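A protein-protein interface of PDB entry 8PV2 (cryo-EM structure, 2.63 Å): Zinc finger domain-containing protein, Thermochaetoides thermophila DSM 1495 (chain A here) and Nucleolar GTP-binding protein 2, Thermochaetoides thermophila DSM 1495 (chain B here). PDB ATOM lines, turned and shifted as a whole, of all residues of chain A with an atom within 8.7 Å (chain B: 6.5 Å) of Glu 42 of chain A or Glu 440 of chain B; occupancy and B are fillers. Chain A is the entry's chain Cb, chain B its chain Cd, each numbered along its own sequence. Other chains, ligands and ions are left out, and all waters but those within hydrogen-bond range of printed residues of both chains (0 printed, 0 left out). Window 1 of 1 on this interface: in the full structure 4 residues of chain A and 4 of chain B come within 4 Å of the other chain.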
ATOM      1  N   LYS A  36       4.986  10.020   5.290  1.00  0.00           N
ATOM      2  CA  LYS A  36       6.249   9.300   5.182  1.00  0.00           C
ATOM      3  C   LYS A  36       7.447  10.200   5.463  1.00  0.00           C
ATOM      4  O   LYS A  36       8.470   9.721   5.965  1.00  0.00           O
ATOM      5  CB  LYS A  36       6.366   8.650   3.808  1.00  0.00           C
ATOM      6  CG  LYS A  36       5.431   7.471   3.625  1.00  0.00           C
ATOM      7  CD  LYS A  36       5.755   6.696   2.367  1.00  0.00           C
ATOM      8  CE  LYS A  36       4.925   5.436   2.278  1.00  0.00           C
ATOM      9  NZ  LYS A  36       5.245   4.650   1.060  1.00  0.00           N
ATOM     10  N   LYS A  39       8.480  10.263   9.039  1.00  0.00           N
ATOM     11  CA  LYS A  39       9.269   9.146   9.532  1.00  0.00           C
ATOM     12  C   LYS A  39      10.667   9.197   8.930  1.00  0.00           C
ATOM     13  O   LYS A  39      10.950   9.989   8.028  1.00  0.00           O
ATOM     14  CB  LYS A  39       8.616   7.801   9.187  1.00  0.00           C
ATOM     15  CG  LYS A  39       7.286   7.536   9.870  1.00  0.00           C
ATOM     16  CD  LYS A  39       7.467   7.168  11.326  1.00  0.00           C
ATOM     17  CE  LYS A  39       6.133   6.870  11.980  1.00  0.00           C
ATOM     18  NZ  LYS A  39       5.997   5.437  12.350  1.00  0.00           N
ATOM     19  N   ALA A  40      11.545   8.343   9.447  1.00  0.00           N
ATOM     20  CA  ALA A  40      12.920   8.232   8.976  1.00  0.00           C
ATOM     21  C   ALA A  40      13.077   6.906   8.247  1.00  0.00           C
ATOM     22  O   ALA A  40      12.814   5.848   8.824  1.00  0.00           O
ATOM     23  CB  ALA A  40      13.907   8.330  10.136  1.00  0.00           C
ATOM     24  N   ALA A  41      13.530   6.967   6.992  1.00  0.00           N
ATOM     25  CA  ALA A  41      13.477   5.797   6.119  1.00  0.00           C
ATOM     26  C   ALA A  41      14.487   4.731   6.525  1.00  0.00           C
ATOM     27  O   ALA A  41      14.245   3.535   6.325  1.00  0.00           O
ATOM     28  CB  ALA A  41      13.708   6.218   4.669  1.00  0.00           C
ATOM     29  N   GLU A  42      15.630   5.137   7.079  1.00  0.00           N
ATOM     30  CA  GLU A  42      16.667   4.168   7.415  1.00  0.00           C
ATOM     31  C   GLU A  42      16.314   3.335   8.641  1.00  0.00           C
ATOM     32  O   GLU A  42      16.877   2.251   8.819  1.00  0.00           O
ATOM     33  CB  GLU A  42      18.005   4.879   7.632  1.00  0.00           C
ATOM     34  CG  GLU A  42      18.077   5.753   8.882  1.00  0.00           C
ATOM     35  CD  GLU A  42      17.531   7.159   8.676  1.00  0.00           C
ATOM     36  OE1 GLU A  42      16.825   7.404   7.677  1.00  0.00           O
ATOM     37  OE2 GLU A  42      17.810   8.027   9.530  1.00  0.00           O
ATOM     38  N   ASP A  43      15.399   3.809   9.481  1.00  0.00           N
ATOM     39  CA  ASP A  43      14.976   3.082  10.669  1.00  0.00           C
ATOM     40  C   ASP A  43      13.703   2.279  10.452  1.00  0.00           C
ATOM     41  O   ASP A  43      13.201   1.672  11.402  1.00  0.00           O
ATOM     42  CB  ASP A  43      14.772   4.054  11.833  1.00  0.00           C
ATOM     43  CG  ASP A  43      16.068   4.678  12.302  1.00  0.00           C
ATOM     44  OD1 ASP A  43      17.136   4.291  11.784  1.00  0.00           O
ATOM     45  OD2 ASP A  43      16.021   5.554  13.189  1.00  0.00           O
ATOM     46  N   LEU A  44      13.173   2.267   9.250  1.00  0.00           N
ATOM     47  CA  LEU A  44      11.952   1.565   8.905  1.00  0.00           C
ATOM     48  C   LEU A  44      12.234   0.095   8.621  1.00  0.00           C
ATOM     49  O   LEU A  44      13.355  -0.266   8.254  1.00  0.00           O
ATOM     50  CB  LEU A  44      11.294   2.207   7.681  1.00  0.00           C
ATOM     51  CG  LEU A  44      10.640   3.559   7.954  1.00  0.00           C
ATOM     52  CD1 LEU A  44      10.155   4.191   6.667  1.00  0.00           C
ATOM     53  CD2 LEU A  44       9.504   3.411   8.944  1.00  0.00           C
ATOM     54  N   PRO A  45      11.244  -0.778   8.812  1.00  0.00           N
ATOM     55  CA  PRO A  45      11.410  -2.177   8.405  1.00  0.00           C
ATOM     56  C   PRO A  45      11.570  -2.291   6.897  1.00  0.00           C
ATOM     57  O   PRO A  45      10.714  -1.848   6.129  1.00  0.00           O
ATOM     58  CB  PRO A  45      10.113  -2.842   8.878  1.00  0.00           C
ATOM     59  CG  PRO A  45       9.551  -1.939   9.898  1.00  0.00           C
ATOM     60  CD  PRO A  45       9.986  -0.562   9.548  1.00  0.00           C
ATOM     61  N   GLY A  46      12.678  -2.894   6.476  1.00  0.00           N
ATOM     62  CA  GLY A  46      12.931  -3.064   5.060  1.00  0.00           C
ATOM     63  C   GLY A  46      13.203  -1.783   4.311  1.00  0.00           C
ATOM     64  O   GLY A  46      12.908  -1.703   3.115  1.00  0.00           O
ATOM     65  N   LEU A  47      13.733  -0.766   4.997  1.00  0.00           N
ATOM     66  CA  LEU A  47      14.113   0.531   4.432  1.00  0.00           C
ATOM     67  C   LEU A  47      12.932   1.279   3.823  1.00  0.00           C
ATOM     68  O   LEU A  47      13.119   2.124   2.944  1.00  0.00           O
ATOM     69  CB  LEU A  47      15.237   0.382   3.400  1.00  0.00           C
ATOM     70  CG  LEU A  47      16.570  -0.088   3.971  1.00  0.00           C
ATOM     71  CD1 LEU A  47      17.535  -0.448   2.860  1.00  0.00           C
ATOM     72  CD2 LEU A  47      17.147   1.003   4.842  1.00  0.00           C
ATOM     73  N   GLY A  48      11.715   0.989   4.275  1.00  0.00           N
ATOM     74  CA  GLY A  48      10.534   1.665   3.789  1.00  0.00           C
ATOM     75  C   GLY A  48      10.051   1.232   2.424  1.00  0.00           C
ATOM     76  O   GLY A  48       9.104   1.832   1.904  1.00  0.00           O
ATOM     77  N   LEU B 429      32.413  -7.840   4.586  1.00  0.00           N
ATOM     78  CA  LEU B 429      31.464  -6.801   4.230  1.00  0.00           C
ATOM     79  C   LEU B 429      32.180  -5.764   3.382  1.00  0.00           C
ATOM     80  O   LEU B 429      33.330  -5.416   3.646  1.00  0.00           O
ATOM     81  CB  LEU B 429      30.879  -6.155   5.491  1.00  0.00           C
ATOM     82  CG  LEU B 429      29.531  -5.453   5.435  1.00  0.00           C
ATOM     83  CD1 LEU B 429      28.411  -6.467   5.462  1.00  0.00           C
ATOM     84  CD2 LEU B 429      29.411  -4.489   6.592  1.00  0.00           C
ATOM     85  N   HIS B 435      30.558   5.657   7.870  1.00  0.00           N
ATOM     86  CA  HIS B 435      30.575   4.772   9.028  1.00  0.00           C
ATOM     87  C   HIS B 435      29.168   4.371   9.451  1.00  0.00           C
ATOM     88  O   HIS B 435      28.960   3.257   9.939  1.00  0.00           O
ATOM     89  CB  HIS B 435      31.328   5.435  10.183  1.00  0.00           C
ATOM     90  CG  HIS B 435      30.689   6.689  10.689  1.00  0.00           C
ATOM     91  ND1 HIS B 435      29.897   6.717  11.816  1.00  0.00           N
ATOM     92  CD2 HIS B 435      30.713   7.956  10.216  1.00  0.00           C
ATOM     93  CE1 HIS B 435      29.474   7.950  12.023  1.00  0.00           C
ATOM     94  NE2 HIS B 435      29.951   8.721  11.063  1.00  0.00           N
ATOM     95  N   ILE B 436      28.186   5.255   9.258  1.00  0.00           N
ATOM     96  CA  ILE B 436      26.807   4.923   9.608  1.00  0.00           C
ATOM     97  C   ILE B 436      26.294   3.790   8.729  1.00  0.00           C
ATOM     98  O   ILE B 436      25.687   2.828   9.217  1.00  0.00           O
ATOM     99  CB  ILE B 436      25.907   6.167   9.505  1.00  0.00           C
ATOM    100  CG1 ILE B 436      26.349   7.227  10.511  1.00  0.00           C
ATOM    101  CG2 ILE B 436      24.453   5.797   9.735  1.00  0.00           C
ATOM    102  CD1 ILE B 436      26.122   6.828  11.949  1.00  0.00           C
ATOM    103  N   GLU B 437      26.549   3.877   7.423  1.00  0.00           N
ATOM    104  CA  GLU B 437      26.129   2.808   6.525  1.00  0.00           C
ATOM    105  C   GLU B 437      26.920   1.534   6.780  1.00  0.00           C
ATOM    106  O   GLU B 437      26.373   0.434   6.676  1.00  0.00           O
ATOM    107  CB  GLU B 437      26.261   3.248   5.068  1.00  0.00           C
ATOM    108  CG  GLU B 437      25.818   2.195   4.067  1.00  0.00           C
ATOM    109  CD  GLU B 437      25.842   2.692   2.645  1.00  0.00           C
ATOM    110  OE1 GLU B 437      26.038   3.905   2.451  1.00  0.00           O
ATOM    111  OE2 GLU B 437      25.668   1.873   1.720  1.00  0.00           O
ATOM    112  N   PHE B 438      28.200   1.663   7.138  1.00  0.00           N
ATOM    113  CA  PHE B 438      28.994   0.492   7.509  1.00  0.00           C
ATOM    114  C   PHE B 438      28.383  -0.232   8.707  1.00  0.00           C
ATOM    115  O   PHE B 438      28.212  -1.460   8.690  1.00  0.00           O
ATOM    116  CB  PHE B 438      30.433   0.923   7.809  1.00  0.00           C
ATOM    117  CG  PHE B 438      31.218  -0.086   8.589  1.00  0.00           C
ATOM    118  CD1 PHE B 438      31.684  -1.235   7.983  1.00  0.00           C
ATOM    119  CD2 PHE B 438      31.489   0.114   9.931  1.00  0.00           C
ATOM    120  CE1 PHE B 438      32.402  -2.165   8.697  1.00  0.00           C
ATOM    121  CE2 PHE B 438      32.203  -0.817  10.649  1.00  0.00           C
ATOM    122  CZ  PHE B 438      32.659  -1.955  10.031  1.00  0.00           C
ATOM    123  N   LEU B 439      28.010   0.525   9.742  1.00  0.00           N
ATOM    124  CA  LEU B 439      27.409  -0.075  10.927  1.00  0.00           C
ATOM    125  C   LEU B 439      26.037  -0.663  10.625  1.00  0.00           C
ATOM    126  O   LEU B 439      25.685  -1.718  11.158  1.00  0.00           O
ATOM    127  CB  LEU B 439      27.312   0.957  12.047  1.00  0.00           C
ATOM    128  CG  LEU B 439      28.640   1.464  12.603  1.00  0.00           C
ATOM    129  CD1 LEU B 439      28.410   2.574  13.591  1.00  0.00           C
ATOM    130  CD2 LEU B 439      29.444   0.350  13.226  1.00  0.00           C
ATOM    131  N   GLU B 440      25.251   0.002   9.772  1.00  0.00           N
ATOM    132  CA  GLU B 440      23.934  -0.520   9.419  1.00  0.00           C
ATOM    133  C   GLU B 440      24.030  -1.818   8.629  1.00  0.00           C
ATOM    134  O   GLU B 440      23.267  -2.759   8.879  1.00  0.00           O
ATOM    135  CB  GLU B 440      23.144   0.525   8.634  1.00  0.00           C
ATOM    136  CG  GLU B 440      22.616   1.661   9.480  1.00  0.00           C
ATOM    137  CD  GLU B 440      22.030   2.779   8.645  1.00  0.00           C
ATOM    138  OE1 GLU B 440      22.098   2.692   7.401  1.00  0.00           O
ATOM    139  OE2 GLU B 440      21.499   3.745   9.231  1.00  0.00           O
ATOM    140  N   MET B 441      24.952  -1.889   7.664  1.00  0.00           N
ATOM    141  CA  MET B 441      25.132  -3.124   6.905  1.00  0.00           C
ATOM    142  C   MET B 441      25.634  -4.250   7.794  1.00  0.00           C
ATOM    143  O   MET B 441      25.186  -5.396   7.667  1.00  0.00           O
ATOM    144  CB  MET B 441      26.079  -2.905   5.724  1.00  0.00           C
ATOM    145  CG  MET B 441      25.603  -1.887   4.704  1.00  0.00           C
ATOM    146  SD  MET B 441      26.734  -1.650   3.316  1.00  0.00           S
ATOM    147  CE  MET B 441      27.499  -3.262   3.196  1.00  0.00           C
ATOM    148  N   LEU B 442      26.556  -3.946   8.711  1.00  0.00           N
ATOM    149  CA  LEU B 442      27.027  -4.972   9.639  1.00  0.00           C
ATOM    150  C   LEU B 442      25.911  -5.441  10.568  1.00  0.00           C
ATOM    151  O   LEU B 442      25.812  -6.634  10.875  1.00  0.00           O
ATOM    152  CB  LEU B 442      28.215  -4.446  10.440  1.00  0.00           C
ATOM    153  CG  LEU B 442      28.936  -5.447  11.344  1.00  0.00           C
ATOM    154  CD1 LEU B 442      29.195  -6.765  10.634  1.00  0.00           C
ATOM    155  CD2 LEU B 442      30.231  -4.849  11.850  1.00  0.00           C
ATOM    156  N   ALA B 443      25.057  -4.517  11.018  1.00  0.00           N
ATOM    157  CA  ALA B 443      23.935  -4.877  11.879  1.00  0.00           C
ATOM    158  C   ALA B 443      22.930  -5.762  11.155  1.00  0.00           C
ATOM    159  O   ALA B 443      22.422  -6.730  11.730  1.00  0.00           O
ATOM    160  CB  ALA B 443      23.248  -3.616  12.396  1.00  0.00           C
ATOM    161  N   ARG B 444      22.622  -5.441   9.895  1.00  0.00           N
ATOM    162  CA  ARG B 444      21.695  -6.276   9.137  1.00  0.00           C
ATOM    163  C   ARG B 444      22.311  -7.627   8.801  1.00  0.00           C
ATOM    164  O   ARG B 444      21.598  -8.630   8.700  1.00  0.00           O
ATOM    165  CB  ARG B 444      21.251  -5.566   7.862  1.00  0.00           C
ATOM    166  CG  ARG B 444      20.455  -4.316   8.107  1.00  0.00           C
ATOM    167  CD  ARG B 444      19.783  -3.837   6.840  1.00  0.00           C
ATOM    168  NE  ARG B 444      19.350  -2.453   6.973  1.00  0.00           N
ATOM    169  CZ  ARG B 444      20.052  -1.412   6.551  1.00  0.00           C
ATOM    170  NH1 ARG B 444      21.195  -1.566   5.904  1.00  0.00           N
ATOM    171  NH2 ARG B 444      19.597  -0.185   6.787  1.00  0.00           N
ATOM    172  N   LYS B 445      23.629  -7.675   8.619  1.00  0.00           N
ATOM    173  CA  LYS B 445      24.276  -8.950   8.347  1.00  0.00           C
ATOM    174  C   LYS B 445      24.288  -9.840   9.581  1.00  0.00           C
ATOM    175  O   LYS B 445      24.029 -11.045   9.487  1.00  0.00           O
ATOM    176  CB  LYS B 445      25.699  -8.720   7.846  1.00  0.00           C
ATOM    177  CG  LYS B 445      26.439 -10.002   7.578  1.00  0.00           C
ATOM    178  CD  LYS B 445      27.920  -9.786   7.443  1.00  0.00           C
ATOM    179  CE  LYS B 445      28.622 -11.123   7.362  1.00  0.00           C
ATOM    180  NZ  LYS B 445      30.090 -10.984   7.446  1.00  0.00           N
ATOM    181  N   GLY B 453      12.963  -4.379  13.226  1.00  0.00           N
ATOM    182  CA  GLY B 453      14.051  -4.575  12.294  1.00  0.00           C
ATOM    183  C   GLY B 453      14.990  -3.401  12.146  1.00  0.00           C
ATOM    184  O   GLY B 453      15.797  -3.392  11.212  1.00  0.00           O
ATOM    185  N   GLU B 454      14.898  -2.408  13.020  1.00  0.00           N
ATOM    186  CA  GLU B 454      15.814  -1.277  12.974  1.00  0.00           C
ATOM    187  C   GLU B 454      17.212  -1.723  13.389  1.00  0.00           C
ATOM    188  O   GLU B 454      17.354  -2.439  14.387  1.00  0.00           O
ATOM    189  CB  GLU B 454      15.318  -0.162  13.889  1.00  0.00           C
ATOM    190  CG  GLU B 454      16.273   1.003  14.026  1.00  0.00           C
ATOM    191  CD  GLU B 454      15.998   1.839  15.254  1.00  0.00           C
ATOM    192  OE1 GLU B 454      15.092   1.471  16.030  1.00  0.00           O
ATOM    193  OE2 GLU B 454      16.692   2.858  15.448  1.00  0.00           O
ATOM    194  N   PRO B 455      18.255  -1.349  12.650  1.00  0.00           N
ATOM    195  CA  PRO B 455      19.615  -1.766  13.015  1.00  0.00           C
ATOM    196  C   PRO B 455      20.084  -1.140  14.323  1.00  0.00           C
ATOM    197  O   PRO B 455      19.721  -0.012  14.660  1.00  0.00           O
ATOM    198  CB  PRO B 455      20.458  -1.292  11.826  1.00  0.00           C
ATOM    199  CG  PRO B 455      19.635  -0.237  11.170  1.00  0.00           C
ATOM    200  CD  PRO B 455      18.221  -0.657  11.352  1.00  0.00           C
ATOM    201  N   VAL B 457      22.954   0.307  15.785  1.00  0.00           N
ATOM    202  CA  VAL B 457      24.260   0.892  15.501  1.00  0.00           C
ATOM    203  C   VAL B 457      25.072   1.065  16.780  1.00  0.00           C
ATOM    204  O   VAL B 457      26.302   0.967  16.756  1.00  0.00           O
ATOM    205  CB  VAL B 457      24.102   2.213  14.723  1.00  0.00           C
ATOM    206  CG1 VAL B 457      23.453   1.946  13.384  1.00  0.00           C
ATOM    207  CG2 VAL B 457      23.265   3.209  15.501  1.00  0.00           C
ATOM    208  N   VAL B 460      26.481  -2.492  17.554  1.00  0.00           N
ATOM    209  CA  VAL B 460      27.467  -2.852  16.539  1.00  0.00           C
ATOM    210  C   VAL B 460      28.736  -2.027  16.711  1.00  0.00           C
ATOM    211  O   VAL B 460      29.850  -2.549  16.582  1.00  0.00           O
ATOM    212  CB  VAL B 460      26.859  -2.708  15.134  1.00  0.00           C
ATOM    213  CG1 VAL B 460      27.908  -2.870  14.066  1.00  0.00           C
ATOM    214  CG2 VAL B 460      25.830  -3.757  14.950  1.00  0.00           C
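OE1 of Glu 440 of chain B lies within salt-bridge range of NH2 of Arg 444 of chain B, at 3.9 Å.
Of the 17 printed residues of chain B, 3 touch a printed residue of chain A.
Printed residues of chain B that touch a printed residue of chain A: Glu 440, Arg 444 and Glu 454.
Among the printed residues, no Asp or Glu carboxylate lies within 4 Å of a Lys or Arg side-chain nitrogen of the other chain.
Printed residues of chain B within 4 Å of Asp 43 of chain A: Glu 454 (3.6 Å).
Of the printed residues of chain B, Leu 47 of chain A touches Arg 444.
Of the printed residues of chain A, Glu 454 of chain B touches Asp 43 (3.6 Å).
Ala 41 of chain A touches none of the printed residues of chain B.
The nearest printed residue of chain B that does not touch Leu 47 of chain A is Glu 440 of chain B (5.8 Å).
OE2 of Glu 440 of chain B touches CG of Glu 42 of chain A (3.98 Å).
OE2 of Glu 454 of chain B touches OD2 of Asp 43 of chain A, at 3.6 Å.
Leu 47 of chain A touches Arg 444 of chain B.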
